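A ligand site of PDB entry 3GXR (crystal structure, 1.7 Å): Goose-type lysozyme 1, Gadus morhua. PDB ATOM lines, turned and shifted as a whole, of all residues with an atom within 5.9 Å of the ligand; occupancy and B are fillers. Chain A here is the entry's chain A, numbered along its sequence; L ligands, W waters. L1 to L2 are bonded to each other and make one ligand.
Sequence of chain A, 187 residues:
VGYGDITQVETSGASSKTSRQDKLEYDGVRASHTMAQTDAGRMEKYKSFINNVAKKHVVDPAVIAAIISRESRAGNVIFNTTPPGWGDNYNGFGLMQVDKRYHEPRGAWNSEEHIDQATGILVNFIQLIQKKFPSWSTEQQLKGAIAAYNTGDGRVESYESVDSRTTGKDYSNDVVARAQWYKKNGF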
ATOM      1  N   GLU A  71       3.772 -27.331  20.177  1.00  0.00           N
ATOM      2  CA  GLU A  71       2.316 -27.345  19.974  1.00  0.00           C
ATOM      3  C   GLU A  71       1.802 -28.712  19.518  1.00  0.00           C
ATOM      4  O   GLU A  71       0.786 -29.167  20.000  1.00  0.00           O
ATOM      5  CB  GLU A  71       1.818 -26.193  19.071  1.00  0.00           C
ATOM      6  CG  GLU A  71       2.043 -24.805  19.698  1.00  0.00           C
ATOM      7  CD  GLU A  71       1.057 -24.542  20.824  1.00  0.00           C
ATOM      8  OE1 GLU A  71       0.127 -25.368  21.138  1.00  0.00           O
ATOM      9  OE2 GLU A  71       1.157 -23.439  21.388  1.00  0.00           O
ATOM     10  N   ASP A  88      -6.287 -29.700  21.927  1.00  0.00           N
ATOM     11  CA  ASP A  88      -6.852 -28.814  22.925  1.00  0.00           C
ATOM     12  C   ASP A  88      -8.405 -28.732  22.864  1.00  0.00           C
ATOM     13  O   ASP A  88      -8.984 -27.647  22.982  1.00  0.00           O
ATOM     14  CB  ASP A  88      -6.256 -27.423  22.806  1.00  0.00           C
ATOM     15  CG  ASP A  88      -6.459 -26.589  24.037  1.00  0.00           C
ATOM     16  OD1 ASP A  88      -7.033 -27.088  25.022  1.00  0.00           O
ATOM     17  OD2 ASP A  88      -6.006 -25.425  24.042  1.00  0.00           O
ATOM     18  N   MET A  96       0.870 -25.469  14.576  1.00  0.00           N
ATOM     19  CA  MET A  96       1.062 -24.474  15.648  1.00  0.00           C
ATOM     20  C   MET A  96      -0.153 -24.231  16.555  1.00  0.00           C
ATOM     21  O   MET A  96      -0.095 -23.399  17.463  1.00  0.00           O
ATOM     22  CB  MET A  96       1.630 -23.166  15.058  1.00  0.00           C
ATOM     23  CG  MET A  96       2.950 -23.430  14.303  1.00  0.00           C
ATOM     24  SD  MET A  96       3.561 -22.044  13.345  1.00  0.00           S
ATOM     25  CE  MET A  96       4.042 -20.963  14.663  1.00  0.00           C
ATOM     26  N   GLN A  97      -1.212 -25.041  16.381  1.00  0.00           N
ATOM     27  CA  GLN A  97      -2.357 -25.009  17.313  1.00  0.00           C
ATOM     28  C   GLN A  97      -2.987 -23.610  17.457  1.00  0.00           C
ATOM     29  O   GLN A  97      -3.096 -23.074  18.567  1.00  0.00           O
ATOM     30  CB  GLN A  97      -1.963 -25.690  18.624  1.00  0.00           C
ATOM     31  CG  GLN A  97      -1.720 -27.208  18.320  1.00  0.00           C
ATOM     32  CD  GLN A  97      -3.011 -27.956  18.172  1.00  0.00           C
ATOM     33  OE1 GLN A  97      -3.419 -28.355  17.051  1.00  0.00           O
ATOM     34  NE2 GLN A  97      -3.753 -27.982  19.246  1.00  0.00           N
ATOM     35  N   VAL A  98      -3.403 -23.007  16.321  1.00  0.00           N
ATOM     36  CA  VAL A  98      -4.206 -21.771  16.338  1.00  0.00           C
ATOM     37  C   VAL A  98      -5.486 -22.087  17.062  1.00  0.00           C
ATOM     38  O   VAL A  98      -6.128 -23.069  16.736  1.00  0.00           O
ATOM     39  CB  VAL A  98      -4.495 -21.277  14.885  1.00  0.00           C
ATOM     40  CG1 VAL A  98      -5.620 -20.180  14.890  1.00  0.00           C
ATOM     41  CG2 VAL A  98      -3.188 -20.749  14.183  1.00  0.00           C
ATOM     42  N   ASP A  99      -5.883 -21.296  18.072  1.00  0.00           N
ATOM     43  CA  ASP A  99      -7.090 -21.551  18.828  1.00  0.00           C
ATOM     44  C   ASP A  99      -8.341 -20.978  18.132  1.00  0.00           C
ATOM     45  O   ASP A  99      -8.449 -19.759  17.931  1.00  0.00           O
ATOM     46  CB  ASP A  99      -6.964 -21.031  20.254  1.00  0.00           C
ATOM     47  CG  ASP A  99      -8.034 -21.603  21.153  1.00  0.00           C
ATOM     48  OD1 ASP A  99      -9.230 -21.478  20.793  1.00  0.00           O
ATOM     49  OD2 ASP A  99      -7.688 -22.195  22.220  1.00  0.00           O
ATOM     50  N   LYS A 100      -9.226 -21.875  17.652  1.00  0.00           N
ATOM     51  CA  LYS A 100     -10.360 -21.425  16.850  1.00  0.00           C
ATOM     52  C   LYS A 100     -11.231 -20.419  17.556  1.00  0.00           C
ATOM     53  O   LYS A 100     -11.999 -19.697  16.926  1.00  0.00           O
ATOM     54  CB  LYS A 100     -11.216 -22.626  16.406  1.00  0.00           C
ATOM     55  CG  LYS A 100     -12.046 -23.248  17.524  1.00  0.00           C
ATOM     56  CD  LYS A 100     -12.705 -24.531  17.036  1.00  0.00           C
ATOM     57  CE  LYS A 100     -13.778 -24.976  18.017  1.00  0.00           C
ATOM     58  NZ  LYS A 100     -14.254 -26.339  17.729  1.00  0.00           N
ATOM     59  N   TYR A 102     -10.473 -17.826  19.063  1.00  0.00           N
ATOM     60  CA  TYR A 102     -10.009 -16.456  18.880  1.00  0.00           C
ATOM     61  C   TYR A 102      -9.680 -16.026  17.414  1.00  0.00           C
ATOM     62  O   TYR A 102      -9.616 -14.798  17.088  1.00  0.00           O
ATOM     63  CB  TYR A 102      -8.814 -16.211  19.817  1.00  0.00           C
ATOM     64  CG  TYR A 102      -9.055 -16.641  21.235  1.00  0.00           C
ATOM     65  CD1 TYR A 102      -9.693 -15.786  22.102  1.00  0.00           C
ATOM     66  CD2 TYR A 102      -8.639 -17.899  21.712  1.00  0.00           C
ATOM     67  CE1 TYR A 102      -9.922 -16.155  23.426  1.00  0.00           C
ATOM     68  CE2 TYR A 102      -8.894 -18.279  23.026  1.00  0.00           C
ATOM     69  CZ  TYR A 102      -9.531 -17.395  23.869  1.00  0.00           C
ATOM     70  OH  TYR A 102      -9.769 -17.708  25.194  1.00  0.00           O
ATOM     71  N   HIS A 103      -9.399 -17.025  16.560  1.00  0.00           N
ATOM     72  CA  HIS A 103      -9.037 -16.827  15.169  1.00  0.00           C
ATOM     73  C   HIS A 103      -9.723 -17.865  14.344  1.00  0.00           C
ATOM     74  O   HIS A 103      -9.739 -19.007  14.765  1.00  0.00           O
ATOM     75  CB  HIS A 103      -7.533 -17.086  15.042  1.00  0.00           C
ATOM     76  CG  HIS A 103      -6.742 -16.553  16.206  1.00  0.00           C
ATOM     77  ND1 HIS A 103      -6.285 -15.259  16.235  1.00  0.00           N
ATOM     78  CD2 HIS A 103      -6.340 -17.123  17.378  1.00  0.00           C
ATOM     79  CE1 HIS A 103      -5.645 -15.030  17.378  1.00  0.00           C
ATOM     80  NE2 HIS A 103      -5.645 -16.153  18.084  1.00  0.00           N
ATOM     81  N   ALA A 118      -0.352 -18.470  12.214  1.00  0.00           N
ATOM     82  CA  ALA A 118       0.048 -18.657  13.575  1.00  0.00           C
ATOM     83  C   ALA A 118       1.228 -17.780  13.902  1.00  0.00           C
ATOM     84  O   ALA A 118       1.294 -17.207  14.982  1.00  0.00           O
ATOM     85  CB  ALA A 118       0.363 -20.144  13.867  1.00  0.00           C
ATOM     86  N   ILE A 121      -0.043 -14.343  14.466  1.00  0.00           N
ATOM     87  CA  ILE A 121      -0.544 -14.256  15.846  1.00  0.00           C
ATOM     88  C   ILE A 121       0.550 -13.950  16.843  1.00  0.00           C
ATOM     89  O   ILE A 121       0.374 -13.134  17.761  1.00  0.00           O
ATOM     90  CB  ILE A 121      -1.411 -15.495  16.231  1.00  0.00           C
ATOM     91  CG1 ILE A 121      -2.658 -15.585  15.328  1.00  0.00           C
ATOM     92  CG2 ILE A 121      -1.698 -15.447  17.774  1.00  0.00           C
ATOM     93  CD1 ILE A 121      -3.371 -16.942  15.310  1.00  0.00           C
ATOM     94  N   ASN A 124       1.574 -10.401  16.613  1.00  0.00           N
ATOM     95  CA  ASN A 124       0.623  -9.522  17.261  1.00  0.00           C
ATOM     96  C   ASN A 124       0.897  -9.539  18.783  1.00  0.00           C
ATOM     97  O   ASN A 124       0.827  -8.501  19.452  1.00  0.00           O
ATOM     98  CB  ASN A 124      -0.791  -9.921  16.908  1.00  0.00           C
ATOM     99  CG  ASN A 124      -1.811  -8.872  17.370  1.00  0.00           C
ATOM    100  OD1 ASN A 124      -1.669  -7.668  17.089  1.00  0.00           O
ATOM    101  ND2 ASN A 124      -2.778  -9.316  18.102  1.00  0.00           N
ATOM    102  N   PHE A 125       1.207 -10.702  19.342  1.00  0.00           N
ATOM    103  CA  PHE A 125       1.517 -10.748  20.808  1.00  0.00           C
ATOM    104  C   PHE A 125       2.824 -10.023  21.188  1.00  0.00           C
ATOM    105  O   PHE A 125       2.939  -9.478  22.282  1.00  0.00           O
ATOM    106  CB  PHE A 125       1.494 -12.158  21.342  1.00  0.00           C
ATOM    107  CG  PHE A 125       0.142 -12.679  21.587  1.00  0.00           C
ATOM    108  CD1 PHE A 125      -0.789 -11.936  22.395  1.00  0.00           C
ATOM    109  CD2 PHE A 125      -0.273 -13.892  21.006  1.00  0.00           C
ATOM    110  CE1 PHE A 125      -2.082 -12.397  22.602  1.00  0.00           C
ATOM    111  CE2 PHE A 125      -1.577 -14.397  21.241  1.00  0.00           C
ATOM    112  CZ  PHE A 125      -2.505 -13.639  22.026  1.00  0.00           C
ATOM    113  N   LEU A 128       1.775  -6.480  21.418  1.00  0.00           N
ATOM    114  CA  LEU A 128       0.947  -6.278  22.601  1.00  0.00           C
ATOM    115  C   LEU A 128       1.821  -6.235  23.874  1.00  0.00           C
ATOM    116  O   LEU A 128       1.663  -5.351  24.771  1.00  0.00           O
ATOM    117  CB  LEU A 128      -0.120  -7.402  22.705  1.00  0.00           C
ATOM    118  CG  LEU A 128      -1.310  -7.266  21.735  1.00  0.00           C
ATOM    119  CD1 LEU A 128      -2.262  -8.486  21.851  1.00  0.00           C
ATOM    120  CD2 LEU A 128      -2.082  -5.935  21.995  1.00  0.00           C
ATOM    121  N   ALA A 148       2.278 -15.385  26.030  1.00  0.00           N
ATOM    122  CA  ALA A 148       0.968 -14.934  25.570  1.00  0.00           C
ATOM    123  C   ALA A 148       0.372 -15.794  24.440  1.00  0.00           C
ATOM    124  O   ALA A 148      -0.858 -16.031  24.350  1.00  0.00           O
ATOM    125  CB  ALA A 148       1.106 -13.448  25.081  1.00  0.00           C
ATOM    126  N   TYR A 149       1.248 -16.337  23.600  1.00  0.00           N
ATOM    127  CA  TYR A 149       0.810 -17.208  22.493  1.00  0.00           C
ATOM    128  C   TYR A 149       0.023 -18.387  23.112  1.00  0.00           C
ATOM    129  O   TYR A 149      -0.936 -18.880  22.545  1.00  0.00           O
ATOM    130  CB  TYR A 149       2.012 -17.661  21.634  1.00  0.00           C
ATOM    131  CG  TYR A 149       1.641 -18.497  20.422  1.00  0.00           C
ATOM    132  CD1 TYR A 149       1.464 -17.903  19.166  1.00  0.00           C
ATOM    133  CD2 TYR A 149       1.449 -19.886  20.560  1.00  0.00           C
ATOM    134  CE1 TYR A 149       1.145 -18.653  18.058  1.00  0.00           C
ATOM    135  CE2 TYR A 149       1.103 -20.677  19.464  1.00  0.00           C
ATOM    136  CZ  TYR A 149       0.918 -20.034  18.264  1.00  0.00           C
ATOM    137  OH  TYR A 149       0.575 -20.775  17.176  1.00  0.00           O
ATOM    138  N   ASN A 150       0.438 -18.820  24.316  1.00  0.00           N
ATOM    139  CA  ASN A 150      -0.319 -19.867  25.025  1.00  0.00           C
ATOM    140  C   ASN A 150      -1.442 -19.416  25.960  1.00  0.00           C
ATOM    141  O   ASN A 150      -2.498 -20.108  26.081  1.00  0.00           O
ATOM    142  CB  ASN A 150       0.665 -20.672  25.842  1.00  0.00           C
ATOM    143  CG  ASN A 150      -0.023 -21.788  26.634  1.00  0.00           C
ATOM    144  OD1 ASN A 150      -0.154 -21.731  27.864  1.00  0.00           O
ATOM    145  ND2 ASN A 150      -0.488 -22.770  25.933  1.00  0.00           N
ATOM    146  N   THR A 151      -1.218 -18.323  26.668  1.00  0.00           N
ATOM    147  CA  THR A 151      -2.131 -17.984  27.760  1.00  0.00           C
ATOM    148  C   THR A 151      -2.881 -16.628  27.599  1.00  0.00           C
ATOM    149  O   THR A 151      -3.775 -16.295  28.402  1.00  0.00           O
ATOM    150  CB  THR A 151      -1.390 -18.043  29.136  1.00  0.00           C
ATOM    151  OG1 THR A 151      -2.364 -18.143  30.200  1.00  0.00           O
ATOM    152  CG2 THR A 151      -0.483 -16.843  29.332  1.00  0.00           C
ATOM    153  N   GLY A 152      -2.521 -15.842  26.611  1.00  0.00           N
ATOM    154  CA  GLY A 152      -3.106 -14.510  26.448  1.00  0.00           C
ATOM    155  C   GLY A 152      -2.179 -13.508  27.111  1.00  0.00           C
ATOM    156  O   GLY A 152      -1.572 -13.827  28.133  1.00  0.00           O
ATOM    157  N   ASP A 153      -2.088 -12.315  26.538  1.00  0.00           N
ATOM    158  CA  ASP A 153      -1.282 -11.238  27.073  1.00  0.00           C
ATOM    159  C   ASP A 153      -1.851 -10.774  28.408  1.00  0.00           C
ATOM    160  O   ASP A 153      -1.118 -10.216  29.258  1.00  0.00           O
ATOM    161  CB  ASP A 153      -1.194 -10.074  26.091  1.00  0.00           C
ATOM    162  CG  ASP A 153      -2.518  -9.449  25.834  1.00  0.00           C
ATOM    163  OD1 ASP A 153      -3.309 -10.040  25.073  1.00  0.00           O
ATOM    164  OD2 ASP A 153      -2.781  -8.348  26.384  1.00  0.00           O
ATOM    165  N   GLY A 154      -3.142 -11.062  28.615  1.00  0.00           N
ATOM    166  CA  GLY A 154      -3.793 -10.704  29.881  1.00  0.00           C
ATOM    167  C   GLY A 154      -3.286 -11.508  31.077  1.00  0.00           C
ATOM    168  O   GLY A 154      -3.283 -10.989  32.207  1.00  0.00           O
ATOM    169  N   ARG A 155      -2.834 -12.756  30.846  1.00  0.00           N
ATOM    170  CA  ARG A 155      -2.237 -13.572  31.919  1.00  0.00           C
ATOM    171  C   ARG A 155      -0.689 -13.583  32.000  1.00  0.00           C
ATOM    172  O   ARG A 155      -0.087 -14.512  32.611  1.00  0.00           O
ATOM    173  CB  ARG A 155      -2.787 -15.002  31.892  1.00  0.00           C
ATOM    174  CG  ARG A 155      -4.329 -15.088  32.138  1.00  0.00           C
ATOM    175  CD  ARG A 155      -4.855 -16.578  32.050  1.00  0.00           C
ATOM    176  NE  ARG A 155      -6.306 -16.649  31.836  1.00  0.00           N
ATOM    177  CZ  ARG A 155      -6.896 -16.826  30.648  1.00  0.00           C
ATOM    178  NH1 ARG A 155      -6.176 -16.983  29.539  1.00  0.00           N
ATOM    179  NH2 ARG A 155      -8.202 -16.847  30.578  1.00  0.00           N
HETATM  180  C1  LIG L   1      -4.361 -19.079  22.995  1.00  0.00           C
HETATM  181  C2  LIG L   1      -4.355 -18.147  21.777  1.00  0.00           C
HETATM  182  C3  LIG L   1      -4.423 -16.668  22.207  1.00  0.00           C
HETATM  183  C4  LIG L   1      -5.467 -16.472  23.316  1.00  0.00           C
HETATM  184  C5  LIG L   1      -5.294 -17.488  24.444  1.00  0.00           C
HETATM  185  C6  LIG L   1      -6.270 -17.217  25.619  1.00  0.00           C
HETATM  186  C7  LIG L   1      -3.404 -18.972  19.666  1.00  0.00           C
HETATM  187  C8  LIG L   1      -2.176 -19.568  18.999  1.00  0.00           C
HETATM  188  N1  LIG L   1      -3.208 -18.423  20.900  1.00  0.00           N
HETATM  189  O1  LIG L   1      -4.519 -20.417  22.586  1.00  0.00           O
HETATM  190  O2  LIG L   1      -4.757 -15.879  21.081  1.00  0.00           O
HETATM  191  O3  LIG L   1      -5.385 -15.207  23.922  1.00  0.00           O
HETATM  192  O4  LIG L   1      -5.373 -18.811  23.969  1.00  0.00           O
HETATM  193  O5  LIG L   1      -5.856 -18.049  26.692  1.00  0.00           O
HETATM  194  O6  LIG L   1      -4.484 -19.024  19.029  1.00  0.00           O
HETATM  195  C1  LG2 L   2      -6.335 -14.272  23.388  1.00  0.00           C
HETATM  196  C2  LG2 L   2      -6.489 -13.162  24.423  1.00  0.00           C
HETATM  197  C3  LG2 L   2      -7.534 -12.179  23.925  1.00  0.00           C
HETATM  198  C4  LG2 L   2      -7.304 -11.757  22.458  1.00  0.00           C
HETATM  199  C5  LG2 L   2      -6.714 -12.812  21.523  1.00  0.00           C
HETATM  200  C6  LG2 L   2      -5.762 -12.051  20.586  1.00  0.00           C
HETATM  201  C7  LG2 L   2      -6.286 -13.343  26.913  1.00  0.00           C
HETATM  202  C8  LG2 L   2      -6.719 -14.109  28.124  1.00  0.00           C
HETATM  203  N1  LG2 L   2      -6.776 -13.762  25.717  1.00  0.00           N
HETATM  204  O1  LG2 L   2      -7.448 -10.988  24.695  1.00  0.00           O
HETATM  205  O2  LG2 L   2      -8.484 -11.161  21.905  1.00  0.00           O
HETATM  206  O3  LG2 L   2      -5.856 -13.714  22.201  1.00  0.00           O
HETATM  207  O4  LG2 L   2      -5.955 -12.556  19.306  1.00  0.00           O
HETATM  208  O5  LG2 L   2      -5.541 -12.413  27.091  1.00  0.00           O
HETATM  209  O   HOH W   1      -2.570 -12.178  18.518  1.00  0.00           O
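Water W1 lies within hydrogen-bond range of the side-chain amide nitrogen of Asn 124, the backbone carbonyl oxygen of Ile 121 and an oxygen (O4) of LG2 L2.
N of Asp 99 is in hydrogen-bond range of O6 of LIG L1 (2.8 Å).
O of Tyr 149 lies within hydrogen-bond range of N1 of LIG L1.
The guanidinium group (NH1) of Arg 155 is in hydrogen-bond range of an oxygen (O5) of LIG L1.
A ring nitrogen (NE2) of His 103 sits at hydrogen-bond distance from an oxygen (O2) of LIG L1 (3.1 Å).
The backbone NH (N) of Gly 154 is in hydrogen-bond range of an oxygen (O5) of LG2 L2 (3.1 Å).
An oxygen (O5) of LIG L1 lies within hydrogen-bond range of the backbone carbonyl oxygen (O) of Thr 151.
N of Asp 153 lies within hydrogen-bond range of O5 of LG2 L2, at 3.5 Å.
Merely in contact with the ligand: Gly 152 (3.3 Å), Phe 125 (3.3 Å), Tyr 102 (3.6 Å), Gln 97 (3.7 Å), Asn 150 (3.7 Å) and Val 98 (3.8 Å).
Hydrophobic or aromatic side chains that line the ligand: Tyr 102, His 103, Phe 125 and Tyr 149.
13 residues have an atom within 4 Å of the ligand: Gln 97, Val 98, Asp 99, Tyr 102, His 103, Phe 125, Tyr 149, Asn 150, Thr 151, Gly 152, Asp 153, Gly 154 and Arg 155.
The nearest printed residue that does not touch the ligand is Ala 148 (4.2 Å).
OH of Tyr 149 lies within hydrogen-bond range of O of Met 96, at 2.7 Å.
The guanidinium group of Arg 155 lies within hydrogen-bond range of the backbone carbonyl oxygen of Thr 151, at 2.7 Å.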
